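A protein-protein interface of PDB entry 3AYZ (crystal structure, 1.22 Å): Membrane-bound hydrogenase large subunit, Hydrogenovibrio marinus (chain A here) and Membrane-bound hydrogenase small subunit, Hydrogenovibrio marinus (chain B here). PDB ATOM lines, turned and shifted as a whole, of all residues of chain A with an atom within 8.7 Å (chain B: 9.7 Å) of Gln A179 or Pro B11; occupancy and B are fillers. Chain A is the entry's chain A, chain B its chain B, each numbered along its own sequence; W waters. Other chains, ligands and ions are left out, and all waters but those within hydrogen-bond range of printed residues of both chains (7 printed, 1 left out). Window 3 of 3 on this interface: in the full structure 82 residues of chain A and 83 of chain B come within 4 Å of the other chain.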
ATOM      1  N   ILE A 171      -4.638 -17.725  13.030  1.00  0.00           N
ATOM      2  CA  ILE A 171      -4.380 -16.648  12.035  1.00  0.00           C
ATOM      3  C   ILE A 171      -5.591 -16.501  11.135  1.00  0.00           C
ATOM      4  O   ILE A 171      -5.940 -15.415  10.731  1.00  0.00           O
ATOM      5  CB  ILE A 171      -3.042 -16.909  11.324  1.00  0.00           C
ATOM      6  CG1 ILE A 171      -1.837 -17.062  12.259  1.00  0.00           C
ATOM      7  CG2 ILE A 171      -2.708 -15.823  10.281  1.00  0.00           C
ATOM      8  CD1 ILE A 171      -1.595 -15.906  13.161  1.00  0.00           C
ATOM      9  N   LYS A 173      -8.726 -16.863  11.979  1.00  0.00           N
ATOM     10  CA  LYS A 173      -9.662 -16.030  12.777  1.00  0.00           C
ATOM     11  C   LYS A 173      -9.333 -14.540  12.766  1.00  0.00           C
ATOM     12  O   LYS A 173     -10.189 -13.668  12.598  1.00  0.00           O
ATOM     13  CB  LYS A 173      -9.714 -16.639  14.170  1.00  0.00           C
ATOM     14  CG  LYS A 173     -10.603 -16.078  15.208  1.00  0.00           C
ATOM     15  CD  LYS A 173     -10.485 -16.855  16.515  1.00  0.00           C
ATOM     16  CE  LYS A 173     -10.321 -15.911  17.732  1.00  0.00           C
ATOM     17  NZ  LYS A 173     -11.324 -16.252  18.810  1.00  0.00           N
ATOM     18  N   PHE A 174      -8.040 -14.268  12.949  1.00  0.00           N
ATOM     19  CA  PHE A 174      -7.512 -12.919  12.894  1.00  0.00           C
ATOM     20  C   PHE A 174      -7.831 -12.259  11.555  1.00  0.00           C
ATOM     21  O   PHE A 174      -8.387 -11.174  11.429  1.00  0.00           O
ATOM     22  CB  PHE A 174      -6.024 -12.982  13.138  1.00  0.00           C
ATOM     23  CG  PHE A 174      -5.306 -11.677  13.144  1.00  0.00           C
ATOM     24  CD1 PHE A 174      -5.290 -10.930  14.294  1.00  0.00           C
ATOM     25  CD2 PHE A 174      -4.609 -11.213  12.045  1.00  0.00           C
ATOM     26  CE1 PHE A 174      -4.571  -9.765  14.373  1.00  0.00           C
ATOM     27  CE2 PHE A 174      -3.945 -10.002  12.086  1.00  0.00           C
ATOM     28  CZ  PHE A 174      -3.957  -9.291  13.248  1.00  0.00           C
ATOM     29  N   VAL A 175      -7.538 -12.953  10.455  1.00  0.00           N
ATOM     30  CA  VAL A 175      -7.851 -12.440   9.135  1.00  0.00           C
ATOM     31  C   VAL A 175      -9.345 -12.293   8.923  1.00  0.00           C
ATOM     32  O   VAL A 175      -9.779 -11.296   8.350  1.00  0.00           O
ATOM     33  CB  VAL A 175      -7.226 -13.363   8.021  1.00  0.00           C
ATOM     34  CG1 VAL A 175      -7.702 -13.027   6.608  1.00  0.00           C
ATOM     35  CG2 VAL A 175      -5.699 -13.288   8.082  1.00  0.00           C
ATOM     36  N   ASP A 176     -10.094 -13.281   9.336  1.00  0.00           N
ATOM     37  CA  ASP A 176     -11.516 -13.252   9.087  1.00  0.00           C
ATOM     38  C   ASP A 176     -12.180 -12.138   9.867  1.00  0.00           C
ATOM     39  O   ASP A 176     -13.275 -11.733   9.508  1.00  0.00           O
ATOM     40  CB  ASP A 176     -12.130 -14.605   9.500  1.00  0.00           C
ATOM     41  CG  ASP A 176     -11.875 -15.718   8.548  1.00  0.00           C
ATOM     42  OD1 ASP A 176     -11.373 -15.444   7.466  1.00  0.00           O
ATOM     43  OD2 ASP A 176     -12.120 -16.878   8.906  1.00  0.00           O
ATOM     44  N   SER A 177     -11.513 -11.615  10.892  1.00  0.00           N
ATOM     45  CA  SER A 177     -12.036 -10.521  11.686  1.00  0.00           C
ATOM     46  C   SER A 177     -12.082  -9.208  10.902  1.00  0.00           C
ATOM     47  O   SER A 177     -12.796  -8.296  11.304  1.00  0.00           O
ATOM     48  CB  SER A 177     -11.234 -10.235  12.911  1.00  0.00           C
ATOM     49  OG  SER A 177     -10.018  -9.551  12.685  1.00  0.00           O
ATOM     50  N   GLY A 178     -11.316  -9.132   9.839  1.00  0.00           N
ATOM     51  CA  GLY A 178     -11.189  -7.941   9.031  1.00  0.00           C
ATOM     52  C   GLY A 178     -10.331  -6.855   9.657  1.00  0.00           C
ATOM     53  O   GLY A 178     -10.213  -5.780   9.015  1.00  0.00           O
ATOM     54  N   GLN A 179      -9.750  -7.103  10.813  1.00  0.00           N
ATOM     55  CA  GLN A 179      -8.833  -6.196  11.477  1.00  0.00           C
ATOM     56  C   GLN A 179      -7.435  -6.788  11.381  1.00  0.00           C
ATOM     57  O   GLN A 179      -7.016  -7.553  12.243  1.00  0.00           O
ATOM     58  CB  GLN A 179      -9.276  -5.939  12.916  1.00  0.00           C
ATOM     59  CG  GLN A 179     -10.625  -5.258  13.040  1.00  0.00           C
ATOM     60  CD  GLN A 179     -10.909  -4.965  14.506  1.00  0.00           C
ATOM     61  OE1 GLN A 179     -11.419  -5.855  15.197  1.00  0.00           O
ATOM     62  NE2 GLN A 179     -10.558  -3.787  14.984  1.00  0.00           N
ATOM     63  N   LEU A 180      -6.781  -6.456  10.284  1.00  0.00           N
ATOM     64  CA  LEU A 180      -5.580  -7.192   9.945  1.00  0.00           C
ATOM     65  C   LEU A 180      -4.319  -6.666  10.608  1.00  0.00           C
ATOM     66  O   LEU A 180      -3.229  -7.297  10.557  1.00  0.00           O
ATOM     67  CB  LEU A 180      -5.396  -7.246   8.408  1.00  0.00           C
ATOM     68  CG  LEU A 180      -6.198  -8.234   7.600  1.00  0.00           C
ATOM     69  CD1 LEU A 180      -5.298  -9.419   7.239  1.00  0.00           C
ATOM     70  CD2 LEU A 180      -7.412  -8.868   8.162  1.00  0.00           C
ATOM     71  N   GLY A 181      -4.391  -5.530  11.328  1.00  0.00           N
ATOM     72  CA  GLY A 181      -3.369  -5.014  12.193  1.00  0.00           C
ATOM     73  C   GLY A 181      -2.040  -4.936  11.471  1.00  0.00           C
ATOM     74  O   GLY A 181      -1.970  -4.319  10.411  1.00  0.00           O
ATOM     75  N   ILE A 182      -1.036  -5.571  12.087  1.00  0.00           N
ATOM     76  CA  ILE A 182       0.342  -5.470  11.583  1.00  0.00           C
ATOM     77  C   ILE A 182       0.501  -6.157  10.239  1.00  0.00           C
ATOM     78  O   ILE A 182       1.572  -5.983   9.624  1.00  0.00           O
ATOM     79  CB  ILE A 182       1.380  -6.077  12.534  1.00  0.00           C
ATOM     80  CG1 ILE A 182       1.121  -7.565  12.822  1.00  0.00           C
ATOM     81  CG2 ILE A 182       1.559  -5.298  13.825  1.00  0.00           C
ATOM     82  CD1 ILE A 182       2.433  -8.212  13.295  1.00  0.00           C
ATOM     83  N   PHE A 183      -0.470  -6.865   9.714  1.00  0.00           N
ATOM     84  CA  PHE A 183      -0.387  -7.460   8.368  1.00  0.00           C
ATOM     85  C   PHE A 183      -1.100  -6.666   7.285  1.00  0.00           C
ATOM     86  O   PHE A 183      -0.993  -6.957   6.097  1.00  0.00           O
ATOM     87  CB  PHE A 183      -0.940  -8.881   8.456  1.00  0.00           C
ATOM     88  CG  PHE A 183      -0.235  -9.895   9.341  1.00  0.00           C
ATOM     89  CD1 PHE A 183       1.076  -9.800   9.733  1.00  0.00           C
ATOM     90  CD2 PHE A 183      -0.947 -11.028   9.795  1.00  0.00           C
ATOM     91  CE1 PHE A 183       1.645 -10.722  10.554  1.00  0.00           C
ATOM     92  CE2 PHE A 183      -0.412 -12.018  10.613  1.00  0.00           C
ATOM     93  CZ  PHE A 183       0.949 -11.864  10.981  1.00  0.00           C
ATOM     94  N   LYS A 184      -1.835  -5.653   7.683  1.00  0.00           N
ATOM     95  CA  LYS A 184      -2.618  -4.803   6.827  1.00  0.00           C
ATOM     96  C   LYS A 184      -1.744  -4.172   5.750  1.00  0.00           C
ATOM     97  O   LYS A 184      -0.740  -3.543   6.084  1.00  0.00           O
ATOM     98  CB  LYS A 184      -3.289  -3.685   7.624  1.00  0.00           C
ATOM     99  CG  LYS A 184      -4.378  -2.919   6.879  1.00  0.00           C
ATOM    100  CD  LYS A 184      -5.195  -2.000   7.744  1.00  0.00           C
ATOM    101  CE  LYS A 184      -6.669  -1.981   7.884  1.00  0.00           C
ATOM    102  NZ  LYS A 184      -7.107  -1.163   9.059  1.00  0.00           N
ATOM    103  N   PRO B  11     -15.321  -6.947  18.035  1.00  0.00           N
ATOM    104  CA  PRO B  11     -14.140  -6.267  17.425  1.00  0.00           C
ATOM    105  C   PRO B  11     -13.255  -5.612  18.452  1.00  0.00           C
ATOM    106  O   PRO B  11     -13.585  -5.057  19.503  1.00  0.00           O
ATOM    107  CB  PRO B  11     -14.665  -5.062  16.623  1.00  0.00           C
ATOM    108  CG  PRO B  11     -15.756  -4.704  17.594  1.00  0.00           C
ATOM    109  CD  PRO B  11     -16.466  -6.054  17.770  1.00  0.00           C
ATOM    110  N   ARG B  12     -12.025  -5.666  18.058  1.00  0.00           N
ATOM    111  CA  ARG B  12     -10.935  -5.363  18.998  1.00  0.00           C
ATOM    112  C   ARG B  12     -10.646  -3.889  18.935  1.00  0.00           C
ATOM    113  O   ARG B  12     -10.667  -3.230  17.873  1.00  0.00           O
ATOM    114  CB  ARG B  12      -9.737  -6.261  18.664  1.00  0.00           C
ATOM    115  CG  ARG B  12      -9.915  -7.731  19.065  1.00  0.00           C
ATOM    116  CD  ARG B  12      -8.833  -8.653  18.544  1.00  0.00           C
ATOM    117  NE  ARG B  12      -8.865  -8.843  17.096  1.00  0.00           N
ATOM    118  CZ  ARG B  12      -8.020  -8.462  16.167  1.00  0.00           C
ATOM    119  NH1 ARG B  12      -6.917  -7.783  16.484  1.00  0.00           N
ATOM    120  NH2 ARG B  12      -8.274  -8.788  14.910  1.00  0.00           N
ATOM    121  N   THR B  13     -10.299  -3.316  20.099  1.00  0.00           N
ATOM    122  CA  THR B  13     -10.024  -1.908  20.214  1.00  0.00           C
ATOM    123  C   THR B  13      -8.907  -1.441  19.283  1.00  0.00           C
ATOM    124  O   THR B  13      -7.799  -1.925  19.444  1.00  0.00           O
ATOM    125  CB  THR B  13      -9.674  -1.528  21.669  1.00  0.00           C
ATOM    126  OG1 THR B  13     -10.815  -1.885  22.515  1.00  0.00           O
ATOM    127  CG2 THR B  13      -9.502  -0.028  21.822  1.00  0.00           C
ATOM    128  N   PRO B  14      -9.147  -0.533  18.365  1.00  0.00           N
ATOM    129  CA  PRO B  14      -8.086  -0.006  17.529  1.00  0.00           C
ATOM    130  C   PRO B  14      -7.092   0.826  18.314  1.00  0.00           C
ATOM    131  O   PRO B  14      -7.445   1.666  19.118  1.00  0.00           O
ATOM    132  CB  PRO B  14      -8.791   0.894  16.497  1.00  0.00           C
ATOM    133  CG  PRO B  14     -10.187   0.390  16.524  1.00  0.00           C
ATOM    134  CD  PRO B  14     -10.453  -0.002  17.954  1.00  0.00           C
ATOM    135  N   VAL B  15      -5.827   0.521  18.077  1.00  0.00           N
ATOM    136  CA  VAL B  15      -4.663   1.196  18.631  1.00  0.00           C
ATOM    137  C   VAL B  15      -3.733   1.621  17.493  1.00  0.00           C
ATOM    138  O   VAL B  15      -3.296   0.820  16.673  1.00  0.00           O
ATOM    139  CB  VAL B  15      -3.929   0.346  19.676  1.00  0.00           C
ATOM    140  CG1 VAL B  15      -2.736   1.097  20.221  1.00  0.00           C
ATOM    141  CG2 VAL B  15      -4.830  -0.072  20.835  1.00  0.00           C
ATOM    142  N   VAL B  42      -1.880  -8.621  20.888  1.00  0.00           N
ATOM    143  CA  VAL B  42      -2.001  -8.200  19.481  1.00  0.00           C
ATOM    144  C   VAL B  42      -2.990  -9.051  18.686  1.00  0.00           C
ATOM    145  O   VAL B  42      -3.705  -8.540  17.786  1.00  0.00           O
ATOM    146  CB  VAL B  42      -0.606  -8.224  18.808  1.00  0.00           C
ATOM    147  CG1 VAL B  42      -0.738  -8.093  17.322  1.00  0.00           C
ATOM    148  CG2 VAL B  42       0.212  -7.080  19.491  1.00  0.00           C
ATOM    149  N   LEU B  43      -3.105 -10.333  19.027  1.00  0.00           N
ATOM    150  CA  LEU B  43      -3.970 -11.212  18.252  1.00  0.00           C
ATOM    151  C   LEU B  43      -5.421 -11.176  18.756  1.00  0.00           C
ATOM    152  O   LEU B  43      -6.370 -11.297  18.007  1.00  0.00           O
ATOM    153  CB  LEU B  43      -3.486 -12.667  18.279  1.00  0.00           C
ATOM    154  CG  LEU B  43      -2.248 -12.941  17.439  1.00  0.00           C
ATOM    155  CD1 LEU B  43      -1.813 -14.404  17.651  1.00  0.00           C
ATOM    156  CD2 LEU B  43      -2.567 -12.744  15.974  1.00  0.00           C
ATOM    157  N   SER B  44      -5.591 -10.935  20.061  1.00  0.00           N
ATOM    158  CA  SER B  44      -6.880 -11.153  20.675  1.00  0.00           C
ATOM    159  C   SER B  44      -7.425 -10.013  21.495  1.00  0.00           C
ATOM    160  O   SER B  44      -8.645 -10.045  21.717  1.00  0.00           O
ATOM    161  CB  SER B  44      -6.737 -12.395  21.614  1.00  0.00           C
ATOM    162  OG  SER B  44      -6.459 -13.547  20.799  1.00  0.00           O
ATOM    163  N   MET B  45      -6.670  -9.030  21.919  1.00  0.00           N
ATOM    164  CA  MET B  45      -7.179  -8.008  22.823  1.00  0.00           C
ATOM    165  C   MET B  45      -7.393  -6.659  22.141  1.00  0.00           C
ATOM    166  O   MET B  45      -8.464  -6.076  22.200  1.00  0.00           O
ATOM    167  CB  MET B  45      -6.259  -7.854  24.046  1.00  0.00           C
ATOM    168  CG  MET B  45      -6.085  -9.152  24.815  1.00  0.00           C
ATOM    169  SD  MET B  45      -5.160  -8.795  26.318  1.00  0.00           S
ATOM    170  CE  MET B  45      -5.247 -10.369  27.073  1.00  0.00           C
ATOM    171  N   ILE B  46      -6.379  -6.171  21.463  1.00  0.00           N
ATOM    172  CA  ILE B  46      -6.444  -4.930  20.723  1.00  0.00           C
ATOM    173  C   ILE B  46      -6.323  -5.263  19.238  1.00  0.00           C
ATOM    174  O   ILE B  46      -6.026  -6.373  18.861  1.00  0.00           O
ATOM    175  CB  ILE B  46      -5.351  -3.953  21.172  1.00  0.00           C
ATOM    176  CG1 ILE B  46      -3.922  -4.438  20.803  1.00  0.00           C
ATOM    177  CG2 ILE B  46      -5.474  -3.602  22.664  1.00  0.00           C
ATOM    178  CD1 ILE B  46      -2.752  -3.508  21.070  1.00  0.00           C
ATOM    179  N   SER B  47      -6.527  -4.222  18.411  1.00  0.00           N
ATOM    180  CA  SER B  47      -6.140  -4.253  17.015  1.00  0.00           C
ATOM    181  C   SER B  47      -5.020  -3.246  16.842  1.00  0.00           C
ATOM    182  O   SER B  47      -5.275  -2.041  16.842  1.00  0.00           O
ATOM    183  CB  SER B  47      -7.297  -3.985  16.024  1.00  0.00           C
ATOM    184  OG  SER B  47      -6.924  -4.207  14.678  1.00  0.00           O
ATOM    185  N   LEU B  48      -3.768  -3.732  16.748  1.00  0.00           N
ATOM    186  CA  LEU B  48      -2.621  -2.853  16.628  1.00  0.00           C
ATOM    187  C   LEU B  48      -2.494  -2.488  15.163  1.00  0.00           C
ATOM    188  O   LEU B  48      -1.953  -3.221  14.319  1.00  0.00           O
ATOM    189  CB  LEU B  48      -1.372  -3.535  17.190  1.00  0.00           C
ATOM    190  CG  LEU B  48      -0.064  -2.711  17.150  1.00  0.00           C
ATOM    191  CD1 LEU B  48      -0.249  -1.468  17.973  1.00  0.00           C
ATOM    192  CD2 LEU B  48       1.123  -3.560  17.619  1.00  0.00           C
ATOM    193  N   ASP B  49      -3.127  -1.365  14.796  1.00  0.00           N
ATOM    194  CA  ASP B  49      -3.353  -1.064  13.416  1.00  0.00           C
ATOM    195  C   ASP B  49      -2.208  -0.308  12.763  1.00  0.00           C
ATOM    196  O   ASP B  49      -2.159  -0.310  11.533  1.00  0.00           O
ATOM    197  CB  ASP B  49      -4.646  -0.256  13.332  1.00  0.00           C
ATOM    198  CG  ASP B  49      -5.844  -1.148  13.604  1.00  0.00           C
ATOM    199  OD1 ASP B  49      -5.791  -2.371  13.463  1.00  0.00           O
ATOM    200  OD2 ASP B  49      -6.885  -0.577  13.933  1.00  0.00           O
ATOM    201  N   TYR B  50      -1.347   0.334  13.543  1.00  0.00           N
ATOM    202  CA  TYR B  50      -0.169   1.017  13.044  1.00  0.00           C
ATOM    203  C   TYR B  50       0.892   0.942  14.117  1.00  0.00           C
ATOM    204  O   TYR B  50       0.576   1.247  15.272  1.00  0.00           O
ATOM    205  CB  TYR B  50      -0.479   2.460  12.693  1.00  0.00           C
ATOM    206  CG  TYR B  50       0.620   3.221  11.966  1.00  0.00           C
ATOM    207  CD1 TYR B  50       0.625   3.308  10.613  1.00  0.00           C
ATOM    208  CD2 TYR B  50       1.612   3.849  12.701  1.00  0.00           C
ATOM    209  CE1 TYR B  50       1.659   4.023  10.023  1.00  0.00           C
ATOM    210  CE2 TYR B  50       2.622   4.568  12.104  1.00  0.00           C
ATOM    211  CZ  TYR B  50       2.644   4.647  10.748  1.00  0.00           C
ATOM    212  OH  TYR B  50       3.675   5.396  10.135  1.00  0.00           O
ATOM    213  N   ILE B  65      -2.732   3.445   5.718  1.00  0.00           N
ATOM    214  CA  ILE B  65      -3.433   2.825   6.847  1.00  0.00           C
ATOM    215  C   ILE B  65      -3.924   3.883   7.815  1.00  0.00           C
ATOM    216  O   ILE B  65      -5.022   3.935   8.334  1.00  0.00           O
ATOM    217  CB  ILE B  65      -2.590   1.792   7.613  1.00  0.00           C
ATOM    218  CG1 ILE B  65      -2.215   0.548   6.809  1.00  0.00           C
ATOM    219  CG2 ILE B  65      -3.279   1.442   8.957  1.00  0.00           C
ATOM    220  CD1 ILE B  65      -1.140  -0.182   7.644  1.00  0.00           C
ATOM    221  N   GLU B  68      -6.858   5.638   6.598  1.00  0.00           N
ATOM    222  CA  GLU B  68      -8.070   4.831   6.631  1.00  0.00           C
ATOM    223  C   GLU B  68      -8.594   4.711   8.063  1.00  0.00           C
ATOM    224  O   GLU B  68      -9.809   4.806   8.348  1.00  0.00           O
ATOM    225  CB  GLU B  68      -7.722   3.485   6.024  1.00  0.00           C
ATOM    226  CG  GLU B  68      -8.813   2.401   5.982  1.00  0.00           C
ATOM    227  CD  GLU B  68      -8.110   1.065   5.728  1.00  0.00           C
ATOM    228  OE1 GLU B  68      -8.136   0.192   6.630  1.00  0.00           O
ATOM    229  OE2 GLU B  68      -7.499   0.936   4.636  1.00  0.00           O
ATOM    230  N   ILE B  69      -7.684   4.420   8.996  1.00  0.00           N
ATOM    231  CA  ILE B  69      -8.130   4.166  10.395  1.00  0.00           C
ATOM    232  C   ILE B  69      -8.806   5.369  11.029  1.00  0.00           C
ATOM    233  O   ILE B  69      -9.830   5.341  11.699  1.00  0.00           O
ATOM    234  CB  ILE B  69      -6.985   3.749  11.347  1.00  0.00           C
ATOM    235  CG1 ILE B  69      -6.500   2.356  11.046  1.00  0.00           C
ATOM    236  CG2 ILE B  69      -7.415   3.927  12.795  1.00  0.00           C
ATOM    237  CD1 ILE B  69      -7.511   1.214  11.116  1.00  0.00           C
ATOM    238  N   LYS B  72     -12.248   5.654   9.367  1.00  0.00           N
ATOM    239  CA  LYS B  72     -13.064   4.492   9.750  1.00  0.00           C
ATOM    240  C   LYS B  72     -13.431   4.464  11.248  1.00  0.00           C
ATOM    241  O   LYS B  72     -14.546   4.137  11.671  1.00  0.00           O
ATOM    242  CB  LYS B  72     -12.310   3.201   9.415  1.00  0.00           C
ATOM    243  CG  LYS B  72     -13.055   1.913   9.788  1.00  0.00           C
ATOM    244  CD  LYS B  72     -12.567   0.649   9.070  1.00  0.00           C
ATOM    245  CE  LYS B  72     -13.560  -0.502   9.174  1.00  0.00           C
ATOM    246  NZ  LYS B  72     -13.340  -1.616   8.198  1.00  0.00           N
ATOM    247  N   TYR B  73     -12.441   4.831  12.063  1.00  0.00           N
ATOM    248  CA  TYR B  73     -12.569   4.720  13.497  1.00  0.00           C
ATOM    249  C   TYR B  73     -12.435   6.083  14.176  1.00  0.00           C
ATOM    250  O   TYR B  73     -11.976   6.145  15.296  1.00  0.00           O
ATOM    251  CB  TYR B  73     -11.502   3.733  14.031  1.00  0.00           C
ATOM    252  CG  TYR B  73     -11.758   2.295  13.563  1.00  0.00           C
ATOM    253  CD1 TYR B  73     -12.725   1.515  14.173  1.00  0.00           C
ATOM    254  CD2 TYR B  73     -11.079   1.652  12.547  1.00  0.00           C
ATOM    255  CE1 TYR B  73     -12.954   0.219  13.746  1.00  0.00           C
ATOM    256  CE2 TYR B  73     -11.280   0.364  12.097  1.00  0.00           C
ATOM    257  CZ  TYR B  73     -12.248  -0.370  12.732  1.00  0.00           C
ATOM    258  OH  TYR B  73     -12.512  -1.655  12.348  1.00  0.00           O
ATOM    259  N   ASN B  76     -12.660   6.717  17.957  1.00  0.00           N
ATOM    260  CA  ASN B  76     -12.746   5.396  18.596  1.00  0.00           C
ATOM    261  C   ASN B  76     -11.425   4.695  18.712  1.00  0.00           C
ATOM    262  O   ASN B  76     -11.382   3.619  19.291  1.00  0.00           O
ATOM    263  CB  ASN B  76     -13.780   4.645  17.793  1.00  0.00           C
ATOM    264  CG  ASN B  76     -15.177   5.167  18.114  1.00  0.00           C
ATOM    265  OD1 ASN B  76     -15.526   5.460  19.261  1.00  0.00           O
ATOM    266  ND2 ASN B  76     -15.930   5.251  17.015  1.00  0.00           N
ATOM    267  N   TYR B  77     -10.327   5.218  18.249  1.00  0.00           N
ATOM    268  CA  TYR B  77      -9.018   4.579  18.436  1.00  0.00           C
ATOM    269  C   TYR B  77      -8.293   5.206  19.608  1.00  0.00           C
ATOM    270  O   TYR B  77      -8.397   6.398  19.926  1.00  0.00           O
ATOM    271  CB  TYR B  77      -8.209   4.639  17.160  1.00  0.00           C
ATOM    272  CG  TYR B  77      -7.886   6.029  16.639  1.00  0.00           C
ATOM    273  CD1 TYR B  77      -6.746   6.691  17.046  1.00  0.00           C
ATOM    274  CD2 TYR B  77      -8.708   6.679  15.710  1.00  0.00           C
ATOM    275  CE1 TYR B  77      -6.399   7.995  16.577  1.00  0.00           C
ATOM    276  CE2 TYR B  77      -8.425   7.932  15.244  1.00  0.00           C
ATOM    277  CZ  TYR B  77      -7.281   8.611  15.665  1.00  0.00           C
ATOM    278  OH  TYR B  77      -7.054   9.845  15.146  1.00  0.00           O
ATOM    279  N   LYS B 113      -9.613   8.779  20.698  1.00  0.00           N
ATOM    280  CA  LYS B 113     -10.505   8.656  21.844  1.00  0.00           C
ATOM    281  C   LYS B 113      -9.825   9.110  23.116  1.00  0.00           C
ATOM    282  O   LYS B 113     -10.345   9.706  24.070  1.00  0.00           O
ATOM    283  CB  LYS B 113     -11.020   7.225  21.929  1.00  0.00           C
ATOM    284  CG  LYS B 113     -11.834   6.816  23.070  1.00  0.00           C
ATOM    285  CD  LYS B 113     -12.119   5.303  23.085  1.00  0.00           C
ATOM    286  CE  LYS B 113     -12.137   4.605  24.406  1.00  0.00           C
ATOM    287  NZ  LYS B 113     -12.605   3.206  24.128  1.00  0.00           N
ATOM    288  N   LEU B 173      -9.515  -2.451  28.925  1.00  0.00           N
ATOM    289  CA  LEU B 173     -10.306  -3.433  28.212  1.00  0.00           C
ATOM    290  C   LEU B 173     -11.263  -4.213  29.128  1.00  0.00           C
ATOM    291  O   LEU B 173     -12.394  -4.570  28.741  1.00  0.00           O
ATOM    292  CB  LEU B 173      -9.457  -4.411  27.440  1.00  0.00           C
ATOM    293  CG  LEU B 173      -8.576  -3.769  26.344  1.00  0.00           C
ATOM    294  CD1 LEU B 173      -7.668  -4.816  25.713  1.00  0.00           C
ATOM    295  CD2 LEU B 173      -9.409  -3.012  25.347  1.00  0.00           C
HETATM  296  O   HOH W   1     -11.299  -3.376   9.771  1.00  0.00           O
HETATM  297  O   HOH W   2      -5.574  -6.523  14.316  1.00  0.00           O
HETATM  298  O   HOH W   3      -1.432  -5.999  14.509  1.00  0.00           O
HETATM  299  O   HOH W   4      -8.855 -13.957  19.097  1.00  0.00           O
HETATM  300  O   HOH W   5      -0.096  -2.341  10.619  1.00  0.00           O
HETATM  301  O   HOH W   6      -3.780  -1.895  10.105  1.00  0.00           O
HETATM  302  O   HOH W   7      -9.216  -1.678  13.456  1.00  0.00           O
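NH2 of Arg B12 sits at hydrogen-bond distance from OG of Ser A177 (2.9 Å).
The backbone NH of Arg B12 lies within hydrogen-bond range of the side-chain amide oxygen of Gln A179 (2.9 Å).
O of Leu B48 is in hydrogen-bond range of N of Ile A182, 3.4 Å away.
OE1 of Glu B68 is in salt-bridge range of NZ of Lys A184, 3.0 Å away.
O of Phe A174 is in hydrogen-bond range of OG of Ser A177, at 2.6 Å.
The side-chain hydroxyl of Ser A177 is in hydrogen-bond range of the backbone NH of Gln A179 (3.1 Å).
The backbone carbonyl oxygen (O) of Ile B46 lies within hydrogen-bond range of the guanidinium group (NH1) of Arg B12 (2.9 Å).
O of Thr B13 lies within hydrogen-bond range of N of Ser B47, 2.8 Å away.
The backbone carbonyl oxygen (O) of Ser B47 sits at hydrogen-bond distance from the backbone NH (N) of Val B15 (2.9 Å).
The backbone carbonyl oxygen of Val B15 lies within hydrogen-bond range of the backbone NH of Asp B49 (2.9 Å).
CD1 of Phe A174 touches NH2 of Arg B12 (3.7 Å).
Phe A174 touches Val B42.
Phe A174 touches Leu B43 (CD1 to CD2, 3.7 Å).
Gln A179 touches Pro B11 (OE1 to CA, 3.5 Å).
OG of Ser B47 touches CB of Gln A179 (3.4 Å).
Gln A179 touches Tyr B73 (NE2 to OH, 3.9 Å).
Gly A181 touches Leu B48.
OD1 of Asp B49 touches CA of Gly A181 (3.8 Å).
Lys A184 touches Ile B65 (O to CD1, 3.7 Å).
Lys A184 touches Ile B69.
Printed residues of chain B within 4 Å of Gln A179: Pro B11 (3.5 Å), Arg B12 (2.9 Å), Ser B47 (3.4 Å) and Tyr B73 (3.9 Å).
Pro B11 touches just one residue of chain A: Gln A179 (3.5 Å).
Of chain B, only Arg B12 (2.9 Å) comes within 4 Å of Ser A177.
No residue of chain B comes within 4 Å of Gly A178.
Printed residues of chain A within 4 Å of Leu B48: Gly A181 (3.1 Å) and Ile A182 (3.4 Å).
Of the printed residues of chain A, Ile B65 touches Lys A184.
Printed residues of chain A within 4 Å of Asp B49: Gly A181 (3.8 Å).
Of the printed residues of chain A, Ile B69 touches Lys A184.
Of the printed residues of chain A, Val B42 touches Phe A174 (3.7 Å).
Ile B46 touches none of the printed residues of chain A.
Phe A183 touches none of the printed residues of chain B.
The nearest residue of chain A that does not touch Pro B11 is Ser A177 (6.5 Å).
The nearest printed residue of chain B that does not touch Lys A184 is Asp B49 (4.7 Å).
Hydrophobic or aromatic side chains of chain B that line the printed part of chain A: Pro B11, Leu B43, Ile B65, Ile B69 and Tyr B73.
Along chain B the printed residues that touch a printed residue of chain A span positions 11 to 73.
Hydrophobic or aromatic side chains of chain A that line the printed part of chain B: Phe A174.
Along chain A the printed residues that touch a printed residue of chain B span positions 174 to 184.
Water W3 bridges the backbone NH of Ile A182 (2.5 Å) and the backbone carbonyl oxygen of Leu B48 (2.8 Å).
Water W6 lies within hydrogen-bond range of O of Asp B49 (2.7 Å) and O of Gly A181 (3.0 Å).
Water W2 lies within hydrogen-bond range of OG of Ser B47 (2.7 Å), O of Gln A179 (2.7 Å), NH1 of Arg B12 (2.8 Å) and N of Gly A181 (3.4 Å).
Water W5 lies within hydrogen-bond range of the backbone carbonyl oxygen of Gly A181 (2.7 Å) and the backbone carbonyl oxygen of Asp B49 (3.0 Å).
Water W1 lies within hydrogen-bond range of O of Gly A178 (2.7 Å), NZ of Lys B72 (3.1 Å) and OH of Tyr B73 (3.3 Å).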
